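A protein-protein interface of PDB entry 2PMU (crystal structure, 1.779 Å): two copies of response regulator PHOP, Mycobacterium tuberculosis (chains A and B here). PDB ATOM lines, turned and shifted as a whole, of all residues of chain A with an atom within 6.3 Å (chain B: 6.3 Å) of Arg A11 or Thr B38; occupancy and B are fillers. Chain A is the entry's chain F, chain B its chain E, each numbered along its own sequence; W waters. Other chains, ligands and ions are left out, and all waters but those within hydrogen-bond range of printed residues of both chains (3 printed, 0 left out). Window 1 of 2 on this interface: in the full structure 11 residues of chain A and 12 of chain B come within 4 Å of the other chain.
The side-chain carboxylate (OE2) of Glu A18 sits at hydrogen-bond distance from the side-chain hydroxyl (OG) of Ser B36 (2.7 Å).
The side-chain hydroxyl (OG1) of Thr B38 lies within hydrogen-bond range of the guanidinium group (NH2) of Arg A11 (2.8 Å).
N of Thr B38 is in hydrogen-bond range of OE1 of Glu A18 (2.9 Å).
The backbone carbonyl oxygen (O) of Val B63 sits at hydrogen-bond distance from the guanidinium group (NH1) of Arg A11.
The side-chain carboxylate (OE2) of Glu A18 sits at hydrogen-bond distance from the side-chain hydroxyl (OH) of Tyr B78 (2.9 Å).
N of Pro B37 sits close to OE1 of Glu A18 (3.5 Å).
The backbone NH of Ser B36 sits at hydrogen-bond distance from the side-chain carboxylate of Glu B39.
OG1 of Thr B41 is in hydrogen-bond range of O of Pro B37, at 3.0 Å.
The side-chain amide nitrogen (ND2) of Asn A9 sits at hydrogen-bond distance from the backbone carbonyl oxygen (O) of Arg A11, at 2.5 Å.
NH2 of Arg B65 touches OD1 of Asn A9 (3.8 Å).
Arg A11 touches Trp B64 (NH2 to CD1, 3.9 Å).
Printed residues of chain B within 4 Å of Asn A9: Arg B65.
Printed residues of chain A within 4 Å of Trp B64: Arg A11 (3.9 Å).
Thr B41 touches none of the printed residues of chain A.
The nearest printed residue of chain B that does not touch Arg A11 is Thr B41 (4.02 Å).
Hydrophobic or aromatic side chains of chain B within 4 Å of the printed part of chain A: Pro B37, Trp B64 and Tyr B78.
Among the printed residues, no Asp or Glu carboxylate lies within 4 Å of a Lys or Arg side-chain nitrogen of the other chain.
No position is printed for both chains.
Of the 8 pairs that touch across the chains among the printed residues, none has its exchanged pair printed and touching as well.
Water W1 lies within hydrogen-bond range of OE1 of Glu A18 (2.7 Å), NE of Arg A11 (2.8 Å) and OG1 of Thr B38 (3.4 Å).
Water W2 bridges the side-chain carboxylate of Glu A18 (2.7 Å) and the side-chain hydroxyl of Tyr B78 (3.2 Å).
Water W3 lies within hydrogen-bond range of the guanidinium group (NH2) of Arg B65 (2.9 Å) and the backbone carbonyl oxygen (O) of Thr A13 (3.0 Å).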
ATOM      1  N   ASN A   9       8.985  18.405  -6.423  1.00  0.00           N
ATOM      2  CA  ASN A   9       7.883  18.621  -7.402  1.00  0.00           C
ATOM      3  C   ASN A   9       8.460  19.285  -8.662  1.00  0.00           C
ATOM      4  O   ASN A   9       8.338  20.506  -8.841  1.00  0.00           O
ATOM      5  CB  ASN A   9       6.772  19.485  -6.773  1.00  0.00           C
ATOM      6  CG  ASN A   9       5.364  19.151  -7.296  1.00  0.00           C
ATOM      7  OD1 ASN A   9       4.381  19.676  -6.786  1.00  0.00           O
ATOM      8  ND2 ASN A   9       5.268  18.281  -8.299  1.00  0.00           N
ATOM      9  N   VAL A  10       9.082  18.462  -9.523  1.00  0.00           N
ATOM     10  CA  VAL A  10       9.795  18.944 -10.729  1.00  0.00           C
ATOM     11  C   VAL A  10       8.959  19.959 -11.505  1.00  0.00           C
ATOM     12  O   VAL A  10       9.462  21.004 -11.925  1.00  0.00           O
ATOM     13  CB  VAL A  10      10.231  17.801 -11.687  1.00  0.00           C
ATOM     14  CG1 VAL A  10       9.033  16.908 -12.109  1.00  0.00           C
ATOM     15  CG2 VAL A  10      10.931  18.398 -12.911  1.00  0.00           C
ATOM     16  N   ARG A  11       7.696  19.608 -11.682  1.00  0.00           N
ATOM     17  CA  ARG A  11       6.662  20.479 -12.181  1.00  0.00           C
ATOM     18  C   ARG A  11       5.876  20.886 -10.918  1.00  0.00           C
ATOM     19  O   ARG A  11       5.456  19.984 -10.183  1.00  0.00           O
ATOM     20  CB  ARG A  11       5.792  19.667 -13.143  1.00  0.00           C
ATOM     21  CG  ARG A  11       4.502  20.318 -13.654  1.00  0.00           C
ATOM     22  CD  ARG A  11       3.703  19.353 -14.601  1.00  0.00           C
ATOM     23  NE  ARG A  11       2.443  19.960 -15.061  1.00  0.00           N
ATOM     24  CZ  ARG A  11       1.348  19.293 -15.417  1.00  0.00           C
ATOM     25  NH1 ARG A  11       1.318  17.966 -15.392  1.00  0.00           N
ATOM     26  NH2 ARG A  11       0.263  19.953 -15.789  1.00  0.00           N
ATOM     27  N   LEU A  12       5.715  22.203 -10.658  1.00  0.00           N
ATOM     28  CA  LEU A  12       4.874  22.750  -9.549  1.00  0.00           C
ATOM     29  C   LEU A  12       3.831  23.760 -10.041  1.00  0.00           C
ATOM     30  O   LEU A  12       4.155  24.617 -10.829  1.00  0.00           O
ATOM     31  CB  LEU A  12       5.762  23.455  -8.502  1.00  0.00           C
ATOM     32  CG  LEU A  12       5.199  23.986  -7.173  1.00  0.00           C
ATOM     33  CD1 LEU A  12       4.699  22.863  -6.218  1.00  0.00           C
ATOM     34  CD2 LEU A  12       6.284  24.814  -6.494  1.00  0.00           C
ATOM     35  N   THR A  13       2.595  23.674  -9.557  1.00  0.00           N
ATOM     36  CA  THR A  13       1.518  24.516 -10.116  1.00  0.00           C
ATOM     37  C   THR A  13       0.495  24.919  -9.069  1.00  0.00           C
ATOM     38  O   THR A  13       0.284  24.202  -8.095  1.00  0.00           O
ATOM     39  CB  THR A  13       0.749  23.794 -11.279  1.00  0.00           C
ATOM     40  OG1 THR A  13       1.598  22.861 -11.927  1.00  0.00           O
ATOM     41  CG2 THR A  13       0.256  24.791 -12.326  1.00  0.00           C
ATOM     42  N   GLU A  18       2.676  28.077 -13.295  1.00  0.00           N
ATOM     43  CA  GLU A  18       3.478  26.847 -13.447  1.00  0.00           C
ATOM     44  C   GLU A  18       4.939  27.157 -13.243  1.00  0.00           C
ATOM     45  O   GLU A  18       5.445  28.123 -13.791  1.00  0.00           O
ATOM     46  CB  GLU A  18       3.325  26.292 -14.860  1.00  0.00           C
ATOM     47  CG  GLU A  18       1.923  25.941 -15.265  1.00  0.00           C
ATOM     48  CD  GLU A  18       1.844  25.483 -16.689  1.00  0.00           C
ATOM     49  OE1 GLU A  18       2.448  24.435 -16.995  1.00  0.00           O
ATOM     50  OE2 GLU A  18       1.085  26.106 -17.453  1.00  0.00           O
ATOM     51  N   LEU A  19       5.633  26.307 -12.485  1.00  0.00           N
ATOM     52  CA  LEU A  19       7.071  26.476 -12.253  1.00  0.00           C
ATOM     53  C   LEU A  19       7.760  25.183 -12.549  1.00  0.00           C
ATOM     54  O   LEU A  19       7.203  24.122 -12.302  1.00  0.00           O
ATOM     55  CB  LEU A  19       7.395  26.817 -10.785  1.00  0.00           C
ATOM     56  CG  LEU A  19       6.941  28.125 -10.148  1.00  0.00           C
ATOM     57  CD1 LEU A  19       5.484  28.059  -9.755  1.00  0.00           C
ATOM     58  CD2 LEU A  19       7.792  28.364  -8.927  1.00  0.00           C
ATOM     59  N   ASP A  20       8.965  25.291 -13.092  1.00  0.00           N
ATOM     60  CA  ASP A  20       9.822  24.124 -13.351  1.00  0.00           C
ATOM     61  C   ASP A  20      11.070  24.345 -12.515  1.00  0.00           C
ATOM     62  O   ASP A  20      11.913  25.176 -12.857  1.00  0.00           O
ATOM     63  CB  ASP A  20      10.167  24.024 -14.837  1.00  0.00           C
ATOM     64  CG  ASP A  20      11.188  22.907 -15.144  1.00  0.00           C
ATOM     65  OD1 ASP A  20      10.849  21.975 -15.901  1.00  0.00           O
ATOM     66  OD2 ASP A  20      12.319  22.977 -14.621  1.00  0.00           O
ATOM     67  N   GLU A  21      11.158  23.615 -11.412  1.00  0.00           N
ATOM     68  CA  GLU A  21      12.294  23.738 -10.473  1.00  0.00           C
ATOM     69  C   GLU A  21      13.665  23.384 -11.063  1.00  0.00           C
ATOM     70  O   GLU A  21      14.678  23.888 -10.574  1.00  0.00           O
ATOM     71  CB  GLU A  21      12.027  22.941  -9.183  1.00  0.00           C
ATOM     72  CG  GLU A  21      10.576  23.086  -8.696  1.00  0.00           C
ATOM     73  CD  GLU A  21      10.401  22.943  -7.201  1.00  0.00           C
ATOM     74  OE1 GLU A  21      10.981  23.749  -6.461  1.00  0.00           O
ATOM     75  OE2 GLU A  21       9.660  22.041  -6.760  1.00  0.00           O
ATOM     76  N   LEU B  35       4.067  25.913 -26.103  1.00  0.00           N
ATOM     77  CA  LEU B  35       3.100  25.507 -25.045  1.00  0.00           C
ATOM     78  C   LEU B  35       3.773  25.444 -23.710  1.00  0.00           C
ATOM     79  O   LEU B  35       4.928  24.983 -23.629  1.00  0.00           O
ATOM     80  CB  LEU B  35       2.542  24.116 -25.339  1.00  0.00           C
ATOM     81  CG  LEU B  35       1.712  23.982 -26.625  1.00  0.00           C
ATOM     82  CD1 LEU B  35       1.010  22.638 -26.636  1.00  0.00           C
ATOM     83  CD2 LEU B  35       0.669  25.081 -26.800  1.00  0.00           C
ATOM     84  N   SER B  36       3.029  25.785 -22.630  1.00  0.00           N
ATOM     85  CA  SER B  36       3.535  25.569 -21.258  1.00  0.00           C
ATOM     86  C   SER B  36       3.416  24.048 -20.994  1.00  0.00           C
ATOM     87  O   SER B  36       2.764  23.359 -21.770  1.00  0.00           O
ATOM     88  CB  SER B  36       2.681  26.330 -20.255  1.00  0.00           C
ATOM     89  OG  SER B  36       1.403  25.696 -20.125  1.00  0.00           O
ATOM     90  N   PRO B  37       4.071  23.522 -19.948  1.00  0.00           N
ATOM     91  CA  PRO B  37       3.975  22.078 -19.659  1.00  0.00           C
ATOM     92  C   PRO B  37       2.551  21.551 -19.487  1.00  0.00           C
ATOM     93  O   PRO B  37       2.218  20.478 -20.021  1.00  0.00           O
ATOM     94  CB  PRO B  37       4.787  21.919 -18.367  1.00  0.00           C
ATOM     95  CG  PRO B  37       5.778  23.015 -18.451  1.00  0.00           C
ATOM     96  CD  PRO B  37       5.010  24.185 -19.029  1.00  0.00           C
ATOM     97  N   THR B  38       1.700  22.330 -18.804  1.00  0.00           N
ATOM     98  CA  THR B  38       0.311  21.941 -18.659  1.00  0.00           C
ATOM     99  C   THR B  38      -0.417  21.915 -20.039  1.00  0.00           C
ATOM    100  O   THR B  38      -1.102  20.950 -20.344  1.00  0.00           O
ATOM    101  CB  THR B  38      -0.438  22.839 -17.666  1.00  0.00           C
ATOM    102  OG1 THR B  38       0.116  22.693 -16.340  1.00  0.00           O
ATOM    103  CG2 THR B  38      -1.907  22.387 -17.605  1.00  0.00           C
ATOM    104  N   GLU B  39      -0.268  22.965 -20.846  1.00  0.00           N
ATOM    105  CA  GLU B  39      -0.830  22.974 -22.211  1.00  0.00           C
ATOM    106  C   GLU B  39      -0.312  21.787 -22.997  1.00  0.00           C
ATOM    107  O   GLU B  39      -1.060  21.154 -23.726  1.00  0.00           O
ATOM    108  CB  GLU B  39      -0.481  24.262 -22.913  1.00  0.00           C
ATOM    109  CG  GLU B  39      -1.170  25.477 -22.310  1.00  0.00           C
ATOM    110  CD  GLU B  39      -0.693  26.771 -22.969  1.00  0.00           C
ATOM    111  OE1 GLU B  39       0.471  26.829 -23.491  1.00  0.00           O
ATOM    112  OE2 GLU B  39      -1.490  27.736 -22.949  1.00  0.00           O
ATOM    113  N   PHE B  40       0.978  21.486 -22.846  1.00  0.00           N
ATOM    114  CA  PHE B  40       1.550  20.320 -23.604  1.00  0.00           C
ATOM    115  C   PHE B  40       0.869  19.023 -23.172  1.00  0.00           C
ATOM    116  O   PHE B  40       0.501  18.199 -24.001  1.00  0.00           O
ATOM    117  CB  PHE B  40       3.077  20.267 -23.438  1.00  0.00           C
ATOM    118  CG  PHE B  40       3.723  19.230 -24.306  1.00  0.00           C
ATOM    119  CD1 PHE B  40       4.165  19.558 -25.589  1.00  0.00           C
ATOM    120  CD2 PHE B  40       3.775  17.907 -23.854  1.00  0.00           C
ATOM    121  CE1 PHE B  40       4.720  18.569 -26.402  1.00  0.00           C
ATOM    122  CE2 PHE B  40       4.329  16.901 -24.629  1.00  0.00           C
ATOM    123  CZ  PHE B  40       4.799  17.259 -25.939  1.00  0.00           C
ATOM    124  N   THR B  41       0.726  18.824 -21.859  1.00  0.00           N
ATOM    125  CA  THR B  41       0.156  17.598 -21.273  1.00  0.00           C
ATOM    126  C   THR B  41      -1.275  17.491 -21.729  1.00  0.00           C
ATOM    127  O   THR B  41      -1.758  16.418 -22.065  1.00  0.00           O
ATOM    128  CB  THR B  41       0.272  17.644 -19.730  1.00  0.00           C
ATOM    129  OG1 THR B  41       1.666  17.635 -19.382  1.00  0.00           O
ATOM    130  CG2 THR B  41      -0.384  16.442 -19.108  1.00  0.00           C
ATOM    131  N   LEU B  42      -1.956  18.631 -21.747  1.00  0.00           N
ATOM    132  CA  LEU B  42      -3.358  18.621 -22.214  1.00  0.00           C
ATOM    133  C   LEU B  42      -3.465  18.243 -23.686  1.00  0.00           C
ATOM    134  O   LEU B  42      -4.290  17.399 -24.088  1.00  0.00           O
ATOM    135  CB  LEU B  42      -3.875  20.058 -22.003  1.00  0.00           C
ATOM    136  CG  LEU B  42      -5.344  20.288 -22.292  1.00  0.00           C
ATOM    137  CD1 LEU B  42      -6.196  19.350 -21.446  1.00  0.00           C
ATOM    138  CD2 LEU B  42      -5.647  21.763 -21.980  1.00  0.00           C
ATOM    139  N   LEU B  43      -2.650  18.873 -24.523  1.00  0.00           N
ATOM    140  CA  LEU B  43      -2.648  18.493 -25.966  1.00  0.00           C
ATOM    141  C   LEU B  43      -2.355  17.019 -26.173  1.00  0.00           C
ATOM    142  O   LEU B  43      -3.014  16.326 -26.987  1.00  0.00           O
ATOM    143  CB  LEU B  43      -1.608  19.325 -26.709  1.00  0.00           C
ATOM    144  CG  LEU B  43      -1.630  19.088 -28.237  1.00  0.00           C
ATOM    145  CD1 LEU B  43      -3.054  19.271 -28.876  1.00  0.00           C
ATOM    146  CD2 LEU B  43      -0.600  19.922 -28.959  1.00  0.00           C
ATOM    147  N   HIS B  62      -6.330  13.555 -15.337  1.00  0.00           N
ATOM    148  CA  HIS B  62      -5.185  13.097 -16.103  1.00  0.00           C
ATOM    149  C   HIS B  62      -4.111  14.089 -16.376  1.00  0.00           C
ATOM    150  O   HIS B  62      -2.926  13.715 -16.527  1.00  0.00           O
ATOM    151  CB  HIS B  62      -5.645  12.475 -17.415  1.00  0.00           C
ATOM    152  CG  HIS B  62      -6.272  11.132 -17.241  1.00  0.00           C
ATOM    153  ND1 HIS B  62      -7.604  10.968 -16.924  1.00  0.00           N
ATOM    154  CD2 HIS B  62      -5.757   9.890 -17.372  1.00  0.00           C
ATOM    155  CE1 HIS B  62      -7.881   9.677 -16.845  1.00  0.00           C
ATOM    156  NE2 HIS B  62      -6.774   9.001 -17.111  1.00  0.00           N
ATOM    157  N   VAL B  63      -4.479  15.355 -16.441  1.00  0.00           N
ATOM    158  CA  VAL B  63      -3.538  16.380 -16.910  1.00  0.00           C
ATOM    159  C   VAL B  63      -2.733  16.996 -15.731  1.00  0.00           C
ATOM    160  O   VAL B  63      -1.620  17.533 -15.915  1.00  0.00           O
ATOM    161  CB  VAL B  63      -4.256  17.428 -17.773  1.00  0.00           C
ATOM    162  CG1 VAL B  63      -3.360  18.671 -18.050  1.00  0.00           C
ATOM    163  CG2 VAL B  63      -4.663  16.827 -19.101  1.00  0.00           C
ATOM    164  N   TRP B  64      -3.264  16.864 -14.521  1.00  0.00           N
ATOM    165  CA  TRP B  64      -2.565  17.333 -13.316  1.00  0.00           C
ATOM    166  C   TRP B  64      -2.546  16.207 -12.310  1.00  0.00           C
ATOM    167  O   TRP B  64      -3.345  15.280 -12.402  1.00  0.00           O
ATOM    168  CB  TRP B  64      -3.343  18.489 -12.703  1.00  0.00           C
ATOM    169  CG  TRP B  64      -3.392  19.758 -13.512  1.00  0.00           C
ATOM    170  CD1 TRP B  64      -2.613  20.885 -13.331  1.00  0.00           C
ATOM    171  CD2 TRP B  64      -4.294  20.062 -14.582  1.00  0.00           C
ATOM    172  NE1 TRP B  64      -2.959  21.862 -14.258  1.00  0.00           N
ATOM    173  CE2 TRP B  64      -3.986  21.382 -15.035  1.00  0.00           C
ATOM    174  CE3 TRP B  64      -5.312  19.339 -15.239  1.00  0.00           C
ATOM    175  CZ2 TRP B  64      -4.682  21.995 -16.088  1.00  0.00           C
ATOM    176  CZ3 TRP B  64      -5.975  19.944 -16.302  1.00  0.00           C
ATOM    177  CH2 TRP B  64      -5.657  21.262 -16.712  1.00  0.00           C
ATOM    178  N   ARG B  65      -1.668  16.297 -11.311  1.00  0.00           N
ATOM    179  CA  ARG B  65      -1.688  15.357 -10.185  1.00  0.00           C
ATOM    180  C   ARG B  65      -2.960  15.554  -9.365  1.00  0.00           C
ATOM    181  O   ARG B  65      -3.466  16.673  -9.247  1.00  0.00           O
ATOM    182  CB  ARG B  65      -0.496  15.591  -9.263  1.00  0.00           C
ATOM    183  CG  ARG B  65       0.850  15.752  -9.944  1.00  0.00           C
ATOM    184  CD  ARG B  65       1.905  16.228  -8.951  1.00  0.00           C
ATOM    185  NE  ARG B  65       1.489  17.430  -8.230  1.00  0.00           N
ATOM    186  CZ  ARG B  65       1.076  17.444  -6.967  1.00  0.00           C
ATOM    187  NH1 ARG B  65       1.042  16.320  -6.254  1.00  0.00           N
ATOM    188  NH2 ARG B  65       0.711  18.594  -6.416  1.00  0.00           N
ATOM    189  N   TYR B  78      -7.551  26.251 -19.291  1.00  0.00           N
ATOM    190  CA  TYR B  78      -6.434  25.729 -20.050  1.00  0.00           C
ATOM    191  C   TYR B  78      -6.843  25.265 -21.443  1.00  0.00           C
ATOM    192  O   TYR B  78      -6.083  25.368 -22.377  1.00  0.00           O
ATOM    193  CB  TYR B  78      -5.719  24.605 -19.303  1.00  0.00           C
ATOM    194  CG  TYR B  78      -4.611  25.140 -18.422  1.00  0.00           C
ATOM    195  CD1 TYR B  78      -3.361  25.446 -18.987  1.00  0.00           C
ATOM    196  CD2 TYR B  78      -4.797  25.355 -17.077  1.00  0.00           C
ATOM    197  CE1 TYR B  78      -2.317  25.960 -18.205  1.00  0.00           C
ATOM    198  CE2 TYR B  78      -3.716  25.868 -16.266  1.00  0.00           C
ATOM    199  CZ  TYR B  78      -2.483  26.148 -16.890  1.00  0.00           C
ATOM    200  OH  TYR B  78      -1.416  26.610 -16.125  1.00  0.00           O
HETATM  201  O   HOH W   1       3.313  22.661 -15.145  1.00  0.00           O
HETATM  202  O   HOH W   2       0.742  28.805 -17.119  1.00  0.00           O
HETATM  203  O   HOH W   3       0.585  21.378  -7.296  1.00  0.00           O
